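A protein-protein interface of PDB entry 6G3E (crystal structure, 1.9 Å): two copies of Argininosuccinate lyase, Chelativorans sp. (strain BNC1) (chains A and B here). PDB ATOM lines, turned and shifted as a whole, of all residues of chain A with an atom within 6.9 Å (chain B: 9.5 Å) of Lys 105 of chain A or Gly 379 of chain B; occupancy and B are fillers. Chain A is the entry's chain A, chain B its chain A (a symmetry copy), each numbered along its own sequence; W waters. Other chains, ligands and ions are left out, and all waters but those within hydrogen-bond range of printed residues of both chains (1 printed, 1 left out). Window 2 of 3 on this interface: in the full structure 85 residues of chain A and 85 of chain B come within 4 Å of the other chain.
OE2 of Glu 64 of chain A lies within salt-bridge range of NZ of Lys 105 of chain A.
The side-chain carboxylate (OD2) of Asp 381 of chain B lies within hydrogen-bond range of the backbone NH (N) of Glu 384 of chain B (3.2 Å).
The side-chain carboxylate (OD2) of Asp 381 of chain B sits at hydrogen-bond distance from the backbone NH (N) of Arg 383 of chain B, 3.0 Å away.
OH of Tyr 88 of chain A lies within hydrogen-bond range of OE2 of Glu 92 of chain A, at 2.8 Å.
The guanidinium group (NE) of Arg 110 of chain A sits at hydrogen-bond distance from a ring nitrogen (ND1) of His 107 of chain A.
A ring nitrogen (ND1) of His 107 of chain A lies within hydrogen-bond range of the side-chain hydroxyl (OH) of Tyr 88 of chain A (3.0 Å).
Lys 105 of chain A touches just these residues of chain B: Gly 379 and Asp 381.
Gly 379 of chain B touches just one residue of chain A: Lys 105 (3.3 Å).
No residue of chain B comes within 4 Å of Ile 108 of chain A.
Printed residues of chain A within 4 Å of Asp 381 of chain B: Ser 101 (3.2 Å), Gly 104 (3.5 Å) and Lys 105 (3.96 Å).
Of the printed residues of chain B, Ser 101 of chain A touches Asp 381.
Glu 64 of chain A touches none of the printed residues of chain B.
Leu 60 of chain A touches none of the printed residues of chain B.
The nearest residue of chain B that does not touch Lys 105 of chain A is Ile 380 of chain B (4.1 Å).
The nearest residue of chain A that does not touch Gly 379 of chain B is Glu 64 of chain A (5.7 Å).
The nearest printed residue of chain B that does not touch Ser 101 of chain A is Tyr 382 of chain B (5.9 Å).
OE1 of Glu 92 of chain A is in salt-bridge range of NE of Arg 383 of chain B, at 2.7 Å.
The backbone carbonyl oxygen (O) of Gly 379 of chain B lies within hydrogen-bond range of the side-chain amino group (NZ) of Lys 105 of chain A (3.3 Å).
Water W1 lies within hydrogen-bond range of the backbone NH (N) of Gly 109 of chain A (2.9 Å) and the side-chain carboxylate (OD1) of Asp 372 of chain B (2.9 Å).
No position is printed for both chains.
Of the 7 pairs that touch across the chains among the printed residues, none has its exchanged pair printed and touching as well.
Among the printed residues, merely in contact across the chains: Ser 101 of chain A with Asp 381 of chain B (3.2 Å), Gly 104 of chain A with Asp 381 of chain B (3.5 Å), Gly 104 of chain A with Tyr 382 of chain B (3.4 Å), Lys 105 of chain A with Asp 381 of chain B (3.96 Å) and His 107 of chain A with Arg 383 of chain B (3.6 Å).
Hydrophobic or aromatic side chains of chain A that line the printed part of chain B: His 107.
Of the 18 printed residues of chain B, 4 touch a printed residue of chain A.
Printed residues of chain B that touch a printed residue of chain A: Gly 379, Asp 381, Tyr 382 and Arg 383.
Hydrophobic or aromatic side chains of chain B that line the printed part of chain A: Tyr 382.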
ATOM      1  N   HIS A  50       4.043  -7.522 -21.127  1.00  0.00           N
ATOM      2  CA  HIS A  50       5.130  -8.145 -20.382  1.00  0.00           C
ATOM      3  C   HIS A  50       4.721  -8.389 -18.927  1.00  0.00           C
ATOM      4  O   HIS A  50       4.898  -9.484 -18.396  1.00  0.00           O
ATOM      5  CB  HIS A  50       6.382  -7.271 -20.443  1.00  0.00           C
ATOM      6  CG  HIS A  50       7.568  -7.871 -19.762  1.00  0.00           C
ATOM      7  ND1 HIS A  50       8.232  -8.972 -20.259  1.00  0.00           N
ATOM      8  CD2 HIS A  50       8.216  -7.522 -18.625  1.00  0.00           C
ATOM      9  CE1 HIS A  50       9.234  -9.279 -19.453  1.00  0.00           C
ATOM     10  NE2 HIS A  50       9.246  -8.415 -18.455  1.00  0.00           N
ATOM     11  N   VAL A  51       4.166  -7.361 -18.296  1.00  0.00           N
ATOM     12  CA  VAL A  51       3.701  -7.461 -16.913  1.00  0.00           C
ATOM     13  C   VAL A  51       2.625  -8.537 -16.763  1.00  0.00           C
ATOM     14  O   VAL A  51       2.657  -9.327 -15.816  1.00  0.00           O
ATOM     15  CB  VAL A  51       3.176  -6.099 -16.422  1.00  0.00           C
ATOM     16  CG1 VAL A  51       2.349  -6.229 -15.146  1.00  0.00           C
ATOM     17  CG2 VAL A  51       4.354  -5.153 -16.198  1.00  0.00           C
ATOM     18  N   LEU A  54       4.329 -11.850 -16.901  1.00  0.00           N
ATOM     19  CA  LEU A  54       5.034 -12.119 -15.648  1.00  0.00           C
ATOM     20  C   LEU A  54       4.054 -12.564 -14.567  1.00  0.00           C
ATOM     21  O   LEU A  54       4.405 -13.341 -13.678  1.00  0.00           O
ATOM     22  CB  LEU A  54       5.802 -10.894 -15.157  1.00  0.00           C
ATOM     23  CG  LEU A  54       6.983 -10.384 -15.992  1.00  0.00           C
ATOM     24  CD1 LEU A  54       7.515  -9.111 -15.367  1.00  0.00           C
ATOM     25  CD2 LEU A  54       8.081 -11.429 -16.111  1.00  0.00           C
ATOM     26  N   ILE A  59       5.786 -14.634 -11.534  1.00  0.00           N
ATOM     27  CA  ILE A  59       6.954 -13.819 -11.225  1.00  0.00           C
ATOM     28  C   ILE A  59       6.520 -12.547 -10.500  1.00  0.00           C
ATOM     29  O   ILE A  59       7.205 -12.076  -9.594  1.00  0.00           O
ATOM     30  CB  ILE A  59       7.748 -13.477 -12.502  1.00  0.00           C
ATOM     31  CG1 ILE A  59       8.433 -14.741 -13.022  1.00  0.00           C
ATOM     32  CG2 ILE A  59       8.798 -12.409 -12.229  1.00  0.00           C
ATOM     33  CD1 ILE A  59       8.831 -14.680 -14.477  1.00  0.00           C
ATOM     34  N   LEU A  60       5.387 -11.991 -10.914  1.00  0.00           N
ATOM     35  CA  LEU A  60       4.722 -10.930 -10.167  1.00  0.00           C
ATOM     36  C   LEU A  60       3.457 -11.479  -9.525  1.00  0.00           C
ATOM     37  O   LEU A  60       2.778 -12.317 -10.110  1.00  0.00           O
ATOM     38  CB  LEU A  60       4.352  -9.746 -11.069  1.00  0.00           C
ATOM     39  CG  LEU A  60       5.454  -9.032 -11.848  1.00  0.00           C
ATOM     40  CD1 LEU A  60       4.837  -7.976 -12.755  1.00  0.00           C
ATOM     41  CD2 LEU A  60       6.459  -8.406 -10.900  1.00  0.00           C
ATOM     42  N   GLU A  64       1.095  -6.857  -7.087  1.00  0.00           N
ATOM     43  CA  GLU A  64       2.175  -6.106  -7.721  1.00  0.00           C
ATOM     44  C   GLU A  64       1.779  -5.676  -9.125  1.00  0.00           C
ATOM     45  O   GLU A  64       1.959  -4.521  -9.516  1.00  0.00           O
ATOM     46  CB  GLU A  64       3.449  -6.950  -7.775  1.00  0.00           C
ATOM     47  CG  GLU A  64       4.116  -7.136  -6.424  1.00  0.00           C
ATOM     48  CD  GLU A  64       5.266  -8.121  -6.461  1.00  0.00           C
ATOM     49  OE1 GLU A  64       5.189  -9.113  -7.219  1.00  0.00           O
ATOM     50  OE2 GLU A  64       6.254  -7.900  -5.729  1.00  0.00           O
ATOM     51  N   ILE A  68       1.411  -1.902 -10.804  1.00  0.00           N
ATOM     52  CA  ILE A  68       2.200  -1.482 -11.961  1.00  0.00           C
ATOM     53  C   ILE A  68       1.287  -1.026 -13.093  1.00  0.00           C
ATOM     54  O   ILE A  68       1.468   0.056 -13.643  1.00  0.00           O
ATOM     55  CB  ILE A  68       3.121  -2.609 -12.461  1.00  0.00           C
ATOM     56  CG1 ILE A  68       4.194  -2.912 -11.414  1.00  0.00           C
ATOM     57  CG2 ILE A  68       3.796  -2.211 -13.783  1.00  0.00           C
ATOM     58  CD1 ILE A  68       4.974  -4.193 -11.673  1.00  0.00           C
ATOM     59  N   TYR A  88      12.872   4.758 -22.292  1.00  0.00           N
ATOM     60  CA  TYR A  88      12.529   3.785 -21.264  1.00  0.00           C
ATOM     61  C   TYR A  88      12.901   4.185 -19.831  1.00  0.00           C
ATOM     62  O   TYR A  88      12.048   4.154 -18.944  1.00  0.00           O
ATOM     63  CB  TYR A  88      13.154   2.418 -21.540  1.00  0.00           C
ATOM     64  CG  TYR A  88      12.789   1.498 -20.407  1.00  0.00           C
ATOM     65  CD1 TYR A  88      11.473   1.078 -20.241  1.00  0.00           C
ATOM     66  CD2 TYR A  88      13.723   1.118 -19.456  1.00  0.00           C
ATOM     67  CE1 TYR A  88      11.107   0.279 -19.187  1.00  0.00           C
ATOM     68  CE2 TYR A  88      13.366   0.308 -18.392  1.00  0.00           C
ATOM     69  CZ  TYR A  88      12.055  -0.104 -18.261  1.00  0.00           C
ATOM     70  OH  TYR A  88      11.687  -0.898 -17.202  1.00  0.00           O
ATOM     71  N   GLU A  92      10.391   4.625 -16.745  1.00  0.00           N
ATOM     72  CA  GLU A  92      10.463   3.752 -15.582  1.00  0.00           C
ATOM     73  C   GLU A  92      10.618   4.565 -14.298  1.00  0.00           C
ATOM     74  O   GLU A  92      10.061   4.205 -13.257  1.00  0.00           O
ATOM     75  CB  GLU A  92      11.624   2.768 -15.729  1.00  0.00           C
ATOM     76  CG  GLU A  92      11.691   1.698 -14.650  1.00  0.00           C
ATOM     77  CD  GLU A  92      13.072   1.061 -14.550  1.00  0.00           C
ATOM     78  OE1 GLU A  92      13.971   1.678 -13.933  1.00  0.00           O
ATOM     79  OE2 GLU A  92      13.259  -0.048 -15.092  1.00  0.00           O
ATOM     80  N   SER A 101       8.625   1.773  -5.430  1.00  0.00           N
ATOM     81  CA  SER A 101       9.708   0.866  -5.801  1.00  0.00           C
ATOM     82  C   SER A 101       9.296  -0.298  -6.702  1.00  0.00           C
ATOM     83  O   SER A 101      10.094  -0.770  -7.511  1.00  0.00           O
ATOM     84  CB  SER A 101      10.351   0.299  -4.534  1.00  0.00           C
ATOM     85  OG  SER A 101      10.949   1.325  -3.765  1.00  0.00           O
ATOM     86  N   VAL A 102       8.060  -0.765  -6.562  1.00  0.00           N
ATOM     87  CA  VAL A 102       7.623  -1.959  -7.275  1.00  0.00           C
ATOM     88  C   VAL A 102       7.695  -1.740  -8.788  1.00  0.00           C
ATOM     89  O   VAL A 102       7.718  -2.693  -9.561  1.00  0.00           O
ATOM     90  CB  VAL A 102       6.187  -2.368  -6.866  1.00  0.00           C
ATOM     91  CG1 VAL A 102       5.154  -1.381  -7.414  1.00  0.00           C
ATOM     92  CG2 VAL A 102       5.883  -3.795  -7.323  1.00  0.00           C
ATOM     93  N   ALA A 103       7.747  -0.475  -9.194  1.00  0.00           N
ATOM     94  CA  ALA A 103       7.891  -0.108 -10.598  1.00  0.00           C
ATOM     95  C   ALA A 103       9.088  -0.809 -11.235  1.00  0.00           C
ATOM     96  O   ALA A 103       9.041  -1.200 -12.400  1.00  0.00           O
ATOM     97  CB  ALA A 103       8.036   1.394 -10.734  1.00  0.00           C
ATOM     98  N   GLY A 104      10.157  -0.963 -10.461  1.00  0.00           N
ATOM     99  CA  GLY A 104      11.374  -1.583 -10.953  1.00  0.00           C
ATOM    100  C   GLY A 104      11.172  -3.011 -11.429  1.00  0.00           C
ATOM    101  O   GLY A 104      11.929  -3.516 -12.261  1.00  0.00           O
ATOM    102  N   LYS A 105      10.140  -3.667 -10.910  1.00  0.00           N
ATOM    103  CA  LYS A 105       9.934  -5.080 -11.191  1.00  0.00           C
ATOM    104  C   LYS A 105       9.364  -5.342 -12.584  1.00  0.00           C
ATOM    105  O   LYS A 105       9.380  -6.478 -13.050  1.00  0.00           O
ATOM    106  CB  LYS A 105       9.011  -5.695 -10.136  1.00  0.00           C
ATOM    107  CG  LYS A 105       9.658  -5.806  -8.768  1.00  0.00           C
ATOM    108  CD  LYS A 105       8.950  -6.835  -7.905  1.00  0.00           C
ATOM    109  CE  LYS A 105       9.765  -7.182  -6.673  1.00  0.00           C
ATOM    110  NZ  LYS A 105       9.129  -8.293  -5.917  1.00  0.00           N
ATOM    111  N   MET A 106       8.868  -4.308 -13.256  1.00  0.00           N
ATOM    112  CA  MET A 106       8.323  -4.511 -14.594  1.00  0.00           C
ATOM    113  C   MET A 106       9.431  -4.870 -15.596  1.00  0.00           C
ATOM    114  O   MET A 106       9.148  -5.364 -16.681  1.00  0.00           O
ATOM    115  CB  MET A 106       7.549  -3.275 -15.067  1.00  0.00           C
ATOM    116  CG  MET A 106       8.377  -2.094 -15.574  1.00  0.00           C
ATOM    117  SD  MET A 106       7.427  -1.150 -16.785  1.00  0.00           S
ATOM    118  CE  MET A 106       8.353   0.386 -16.828  1.00  0.00           C
ATOM    119  N   HIS A 107      10.689  -4.634 -15.227  1.00  0.00           N
ATOM    120  CA  HIS A 107      11.804  -4.883 -16.140  1.00  0.00           C
ATOM    121  C   HIS A 107      12.449  -6.255 -15.943  1.00  0.00           C
ATOM    122  O   HIS A 107      13.428  -6.586 -16.619  1.00  0.00           O
ATOM    123  CB  HIS A 107      12.871  -3.793 -15.984  1.00  0.00           C
ATOM    124  CG  HIS A 107      13.602  -3.479 -17.253  1.00  0.00           C
ATOM    125  ND1 HIS A 107      12.958  -3.320 -18.464  1.00  0.00           N
ATOM    126  CD2 HIS A 107      14.919  -3.281 -17.503  1.00  0.00           C
ATOM    127  CE1 HIS A 107      13.846  -3.048 -19.403  1.00  0.00           C
ATOM    128  NE2 HIS A 107      15.045  -3.011 -18.845  1.00  0.00           N
ATOM    129  N   ILE A 108      11.918  -7.044 -15.011  1.00  0.00           N
ATOM    130  CA  ILE A 108      12.410  -8.401 -14.796  1.00  0.00           C
ATOM    131  C   ILE A 108      12.386  -9.205 -16.102  1.00  0.00           C
ATOM    132  O   ILE A 108      11.371  -9.261 -16.790  1.00  0.00           O
ATOM    133  CB  ILE A 108      11.577  -9.130 -13.704  1.00  0.00           C
ATOM    134  CG1 ILE A 108      11.918  -8.560 -12.322  1.00  0.00           C
ATOM    135  CG2 ILE A 108      11.849 -10.631 -13.704  1.00  0.00           C
ATOM    136  CD1 ILE A 108      10.899  -8.886 -11.239  1.00  0.00           C
ATOM    137  N   GLY A 109      13.519  -9.811 -16.445  1.00  0.00           N
ATOM    138  CA  GLY A 109      13.611 -10.644 -17.631  1.00  0.00           C
ATOM    139  C   GLY A 109      13.594  -9.877 -18.947  1.00  0.00           C
ATOM    140  O   GLY A 109      13.355 -10.465 -20.002  1.00  0.00           O
ATOM    141  N   ARG A 110      13.879  -8.579 -18.893  1.00  0.00           N
ATOM    142  CA  ARG A 110      13.723  -7.713 -20.059  1.00  0.00           C
ATOM    143  C   ARG A 110      14.850  -6.687 -20.155  1.00  0.00           C
ATOM    144  O   ARG A 110      15.535  -6.402 -19.171  1.00  0.00           O
ATOM    145  CB  ARG A 110      12.365  -7.008 -19.999  1.00  0.00           C
ATOM    146  CG  ARG A 110      11.957  -6.270 -21.264  1.00  0.00           C
ATOM    147  CD  ARG A 110      10.574  -5.651 -21.093  1.00  0.00           C
ATOM    148  NE  ARG A 110      10.587  -4.584 -20.097  1.00  0.00           N
ATOM    149  CZ  ARG A 110       9.566  -3.774 -19.856  1.00  0.00           C
ATOM    150  NH1 ARG A 110       8.437  -3.910 -20.537  1.00  0.00           N
ATOM    151  NH2 ARG A 110       9.674  -2.828 -18.937  1.00  0.00           N
ATOM    152  N   THR B 371      22.397  -9.926 -10.111  1.00  0.00           N
ATOM    153  CA  THR B 371      21.295  -8.993  -9.924  1.00  0.00           C
ATOM    154  C   THR B 371      19.963  -9.739  -9.830  1.00  0.00           C
ATOM    155  O   THR B 371      19.138  -9.441  -8.966  1.00  0.00           O
ATOM    156  CB  THR B 371      21.230  -7.968 -11.077  1.00  0.00           C
ATOM    157  OG1 THR B 371      22.537  -7.442 -11.324  1.00  0.00           O
ATOM    158  CG2 THR B 371      20.292  -6.827 -10.738  1.00  0.00           C
ATOM    159  N   ASP B 372      19.760 -10.707 -10.722  1.00  0.00           N
ATOM    160  CA  ASP B 372      18.534 -11.499 -10.732  1.00  0.00           C
ATOM    161  C   ASP B 372      18.389 -12.279  -9.430  1.00  0.00           C
ATOM    162  O   ASP B 372      17.285 -12.425  -8.900  1.00  0.00           O
ATOM    163  CB  ASP B 372      18.513 -12.475 -11.919  1.00  0.00           C
ATOM    164  CG  ASP B 372      18.220 -11.785 -13.247  1.00  0.00           C
ATOM    165  OD1 ASP B 372      17.542 -10.737 -13.241  1.00  0.00           O
ATOM    166  OD2 ASP B 372      18.661 -12.296 -14.300  1.00  0.00           O
ATOM    167  N   MET B 373      19.512 -12.780  -8.924  1.00  0.00           N
ATOM    168  CA  MET B 373      19.513 -13.574  -7.706  1.00  0.00           C
ATOM    169  C   MET B 373      19.097 -12.729  -6.508  1.00  0.00           C
ATOM    170  O   MET B 373      18.392 -13.213  -5.624  1.00  0.00           O
ATOM    171  CB  MET B 373      20.892 -14.192  -7.478  1.00  0.00           C
ATOM    172  CG  MET B 373      20.985 -15.069  -6.242  1.00  0.00           C
ATOM    173  SD  MET B 373      21.355 -14.127  -4.753  1.00  0.00           S
ATOM    174  CE  MET B 373      23.104 -13.830  -4.983  1.00  0.00           C
ATOM    175  N   LEU B 374      19.520 -11.469  -6.478  1.00  0.00           N
ATOM    176  CA  LEU B 374      19.124 -10.575  -5.392  1.00  0.00           C
ATOM    177  C   LEU B 374      17.611 -10.376  -5.414  1.00  0.00           C
ATOM    178  O   LEU B 374      16.943 -10.502  -4.392  1.00  0.00           O
ATOM    179  CB  LEU B 374      19.836  -9.223  -5.491  1.00  0.00           C
ATOM    180  CG  LEU B 374      21.360  -9.188  -5.311  1.00  0.00           C
ATOM    181  CD1 LEU B 374      21.834  -7.737  -5.329  1.00  0.00           C
ATOM    182  CD2 LEU B 374      21.815  -9.880  -4.033  1.00  0.00           C
ATOM    183  N   VAL B 375      17.073 -10.081  -6.592  1.00  0.00           N
ATOM    184  CA  VAL B 375      15.635  -9.896  -6.753  1.00  0.00           C
ATOM    185  C   VAL B 375      14.873 -11.142  -6.328  1.00  0.00           C
ATOM    186  O   VAL B 375      13.881 -11.062  -5.605  1.00  0.00           O
ATOM    187  CB  VAL B 375      15.276  -9.564  -8.216  1.00  0.00           C
ATOM    188  CG1 VAL B 375      13.756  -9.493  -8.412  1.00  0.00           C
ATOM    189  CG2 VAL B 375      15.927  -8.257  -8.628  1.00  0.00           C
ATOM    190  N   ARG B 376      15.346 -12.293  -6.787  1.00  0.00           N
ATOM    191  CA  ARG B 376      14.686 -13.556  -6.506  1.00  0.00           C
ATOM    192  C   ARG B 376      14.778 -13.938  -5.029  1.00  0.00           C
ATOM    193  O   ARG B 376      13.801 -14.421  -4.465  1.00  0.00           O
ATOM    194  CB  ARG B 376      15.291 -14.662  -7.370  1.00  0.00           C
ATOM    195  CG  ARG B 376      14.326 -15.780  -7.717  1.00  0.00           C
ATOM    196  CD  ARG B 376      15.007 -16.872  -8.525  1.00  0.00           C
ATOM    197  NE  ARG B 376      16.252 -17.303  -7.888  1.00  0.00           N
ATOM    198  CZ  ARG B 376      17.477 -17.100  -8.376  1.00  0.00           C
ATOM    199  NH1 ARG B 376      17.662 -16.483  -9.543  1.00  0.00           N
ATOM    200  NH2 ARG B 376      18.532 -17.533  -7.696  1.00  0.00           N
ATOM    201  N   ARG B 377      15.936 -13.718  -4.405  1.00  0.00           N
ATOM    202  CA  ARG B 377      16.158 -14.166  -3.026  1.00  0.00           C
ATOM    203  C   ARG B 377      15.608 -13.208  -1.964  1.00  0.00           C
ATOM    204  O   ARG B 377      15.049 -13.668  -0.968  1.00  0.00           O
ATOM    205  CB  ARG B 377      17.652 -14.397  -2.769  1.00  0.00           C
ATOM    206  CG  ARG B 377      18.230 -15.638  -3.446  1.00  0.00           C
ATOM    207  CD  ARG B 377      17.788 -16.939  -2.784  1.00  0.00           C
ATOM    208  NE  ARG B 377      17.657 -18.010  -3.771  1.00  0.00           N
ATOM    209  CZ  ARG B 377      16.503 -18.441  -4.284  1.00  0.00           C
ATOM    210  NH1 ARG B 377      15.342 -17.919  -3.893  1.00  0.00           N
ATOM    211  NH2 ARG B 377      16.509 -19.414  -5.188  1.00  0.00           N
ATOM    212  N   VAL B 378      15.762 -11.914  -2.176  1.00  0.00           N
ATOM    213  CA  VAL B 378      15.366 -10.914  -1.211  1.00  0.00           C
ATOM    214  C   VAL B 378      14.204 -10.027  -1.604  1.00  0.00           C
ATOM    215  O   VAL B 378      13.730  -9.261  -0.816  1.00  0.00           O
ATOM    216  CB  VAL B 378      16.519 -10.013  -0.790  1.00  0.00           C
ATOM    217  CG1 VAL B 378      17.724 -10.827  -0.434  1.00  0.00           C
ATOM    218  CG2 VAL B 378      16.861  -9.002  -1.824  1.00  0.00           C
ATOM    219  N   GLY B 379      13.779 -10.137  -2.834  1.00  0.00           N
ATOM    220  CA  GLY B 379      12.558  -9.491  -3.290  1.00  0.00           C
ATOM    221  C   GLY B 379      12.653  -8.009  -3.600  1.00  0.00           C
ATOM    222  O   GLY B 379      11.632  -7.385  -3.891  1.00  0.00           O
ATOM    223  N   ILE B 380      13.853  -7.435  -3.536  1.00  0.00           N
ATOM    224  CA  ILE B 380      14.028  -6.034  -3.916  1.00  0.00           C
ATOM    225  C   ILE B 380      13.744  -5.880  -5.408  1.00  0.00           C
ATOM    226  O   ILE B 380      13.797  -6.858  -6.153  1.00  0.00           O
ATOM    227  CB  ILE B 380      15.442  -5.513  -3.588  1.00  0.00           C
ATOM    228  CG1 ILE B 380      16.513  -6.400  -4.230  1.00  0.00           C
ATOM    229  CG2 ILE B 380      15.637  -5.440  -2.075  1.00  0.00           C
ATOM    230  CD1 ILE B 380      17.920  -5.832  -4.129  1.00  0.00           C
ATOM    231  N   ASP B 381      13.429  -4.660  -5.840  1.00  0.00           N
ATOM    232  CA  ASP B 381      13.035  -4.433  -7.228  1.00  0.00           C
ATOM    233  C   ASP B 381      14.273  -4.421  -8.110  1.00  0.00           C
ATOM    234  O   ASP B 381      15.385  -4.224  -7.614  1.00  0.00           O
ATOM    235  CB  ASP B 381      12.263  -3.122  -7.371  1.00  0.00           C
ATOM    236  CG  ASP B 381      13.150  -1.906  -7.221  1.00  0.00           C
ATOM    237  OD1 ASP B 381      13.340  -1.445  -6.076  1.00  0.00           O
ATOM    238  OD2 ASP B 381      13.656  -1.413  -8.250  1.00  0.00           O
ATOM    239  N   TYR B 382      14.089  -4.627  -9.412  1.00  0.00           N
ATOM    240  CA  TYR B 382      15.235  -4.819 -10.281  1.00  0.00           C
ATOM    241  C   TYR B 382      16.139  -3.595 -10.337  1.00  0.00           C
ATOM    242  O   TYR B 382      17.360  -3.741 -10.393  1.00  0.00           O
ATOM    243  CB  TYR B 382      14.819  -5.186 -11.708  1.00  0.00           C
ATOM    244  CG  TYR B 382      16.011  -5.734 -12.447  1.00  0.00           C
ATOM    245  CD1 TYR B 382      16.375  -7.061 -12.301  1.00  0.00           C
ATOM    246  CD2 TYR B 382      16.819  -4.911 -13.227  1.00  0.00           C
ATOM    247  CE1 TYR B 382      17.486  -7.571 -12.933  1.00  0.00           C
ATOM    248  CE2 TYR B 382      17.934  -5.413 -13.870  1.00  0.00           C
ATOM    249  CZ  TYR B 382      18.263  -6.746 -13.717  1.00  0.00           C
ATOM    250  OH  TYR B 382      19.375  -7.253 -14.350  1.00  0.00           O
ATOM    251  N   ARG B 383      15.560  -2.395 -10.330  1.00  0.00           N
ATOM    252  CA  ARG B 383      16.367  -1.187 -10.452  1.00  0.00           C
ATOM    253  C   ARG B 383      17.289  -1.013  -9.243  1.00  0.00           C
ATOM    254  O   ARG B 383      18.434  -0.597  -9.402  1.00  0.00           O
ATOM    255  CB  ARG B 383      15.481   0.050 -10.637  1.00  0.00           C
ATOM    256  CG  ARG B 383      16.246   1.327 -10.980  1.00  0.00           C
ATOM    257  CD  ARG B 383      17.120   1.151 -12.221  1.00  0.00           C
ATOM    258  NE  ARG B 383      16.367   0.580 -13.336  1.00  0.00           N
ATOM    259  CZ  ARG B 383      16.837  -0.318 -14.199  1.00  0.00           C
ATOM    260  NH1 ARG B 383      18.086  -0.762 -14.113  1.00  0.00           N
ATOM    261  NH2 ARG B 383      16.052  -0.766 -15.173  1.00  0.00           N
ATOM    262  N   GLU B 384      16.820  -1.347  -8.042  1.00  0.00           N
ATOM    263  CA  GLU B 384      17.681  -1.214  -6.863  1.00  0.00           C
ATOM    264  C   GLU B 384      18.764  -2.298  -6.830  1.00  0.00           C
ATOM    265  O   GLU B 384      19.904  -2.023  -6.455  1.00  0.00           O
ATOM    266  CB  GLU B 384      16.875  -1.268  -5.562  1.00  0.00           C
ATOM    267  CG  GLU B 384      17.693  -0.790  -4.359  1.00  0.00           C
ATOM    268  CD  GLU B 384      17.047  -1.095  -3.016  1.00  0.00           C
ATOM    269  OE1 GLU B 384      15.988  -1.759  -2.988  1.00  0.00           O
ATOM    270  OE2 GLU B 384      17.605  -0.668  -1.983  1.00  0.00           O
ATOM    271  N   ALA B 385      18.411  -3.526  -7.207  1.00  0.00           N
ATOM    272  CA  ALA B 385      19.392  -4.609  -7.281  1.00  0.00           C
ATOM    273  C   ALA B 385      20.493  -4.241  -8.268  1.00  0.00           C
ATOM    274  O   ALA B 385      21.679  -4.455  -8.017  1.00  0.00           O
ATOM    275  CB  ALA B 385      18.733  -5.915  -7.692  1.00  0.00           C
ATOM    276  N   ILE B 423      22.341  -7.008   2.873  1.00  0.00           N
ATOM    277  CA  ILE B 423      21.453  -7.793   2.056  1.00  0.00           C
ATOM    278  C   ILE B 423      21.608  -9.245   2.441  1.00  0.00           C
ATOM    279  O   ILE B 423      22.663  -9.700   2.731  1.00  0.00           O
ATOM    280  CB  ILE B 423      21.709  -7.548   0.556  1.00  0.00           C
ATOM    281  CG1 ILE B 423      20.629  -8.161  -0.313  1.00  0.00           C
ATOM    282  CG2 ILE B 423      23.049  -8.051   0.165  1.00  0.00           C
ATOM    283  CD1 ILE B 423      20.049  -7.192  -1.296  1.00  0.00           C
ATOM    284  N   ASN B 424      20.504  -9.950   2.468  1.00  0.00           N
ATOM    285  CA  ASN B 424      20.432 -11.244   3.125  1.00  0.00           C
ATOM    286  C   ASN B 424      20.534 -12.396   2.127  1.00  0.00           C
ATOM    287  O   ASN B 424      19.537 -13.020   1.763  1.00  0.00           O
ATOM    288  CB  ASN B 424      19.136 -11.318   3.940  1.00  0.00           C
ATOM    289  CG  ASN B 424      19.275 -12.161   5.182  1.00  0.00           C
ATOM    290  OD1 ASN B 424      18.539 -13.128   5.374  1.00  0.00           O
ATOM    291  ND2 ASN B 424      20.227 -11.799   6.040  1.00  0.00           N
ATOM    292  N   VAL B 425      21.762 -12.655   1.684  1.00  0.00           N
ATOM    293  CA  VAL B 425      22.062 -13.763   0.782  1.00  0.00           C
ATOM    294  C   VAL B 425      23.344 -14.442   1.250  1.00  0.00           C
ATOM    295  O   VAL B 425      24.136 -13.841   1.978  1.00  0.00           O
ATOM    296  CB  VAL B 425      22.224 -13.294  -0.684  1.00  0.00           C
ATOM    297  CG1 VAL B 425      20.938 -12.651  -1.189  1.00  0.00           C
ATOM    298  CG2 VAL B 425      23.393 -12.328  -0.823  1.00  0.00           C
HETATM  299  O   HOH W   1      16.257  -9.505 -15.592  1.00  0.00           O
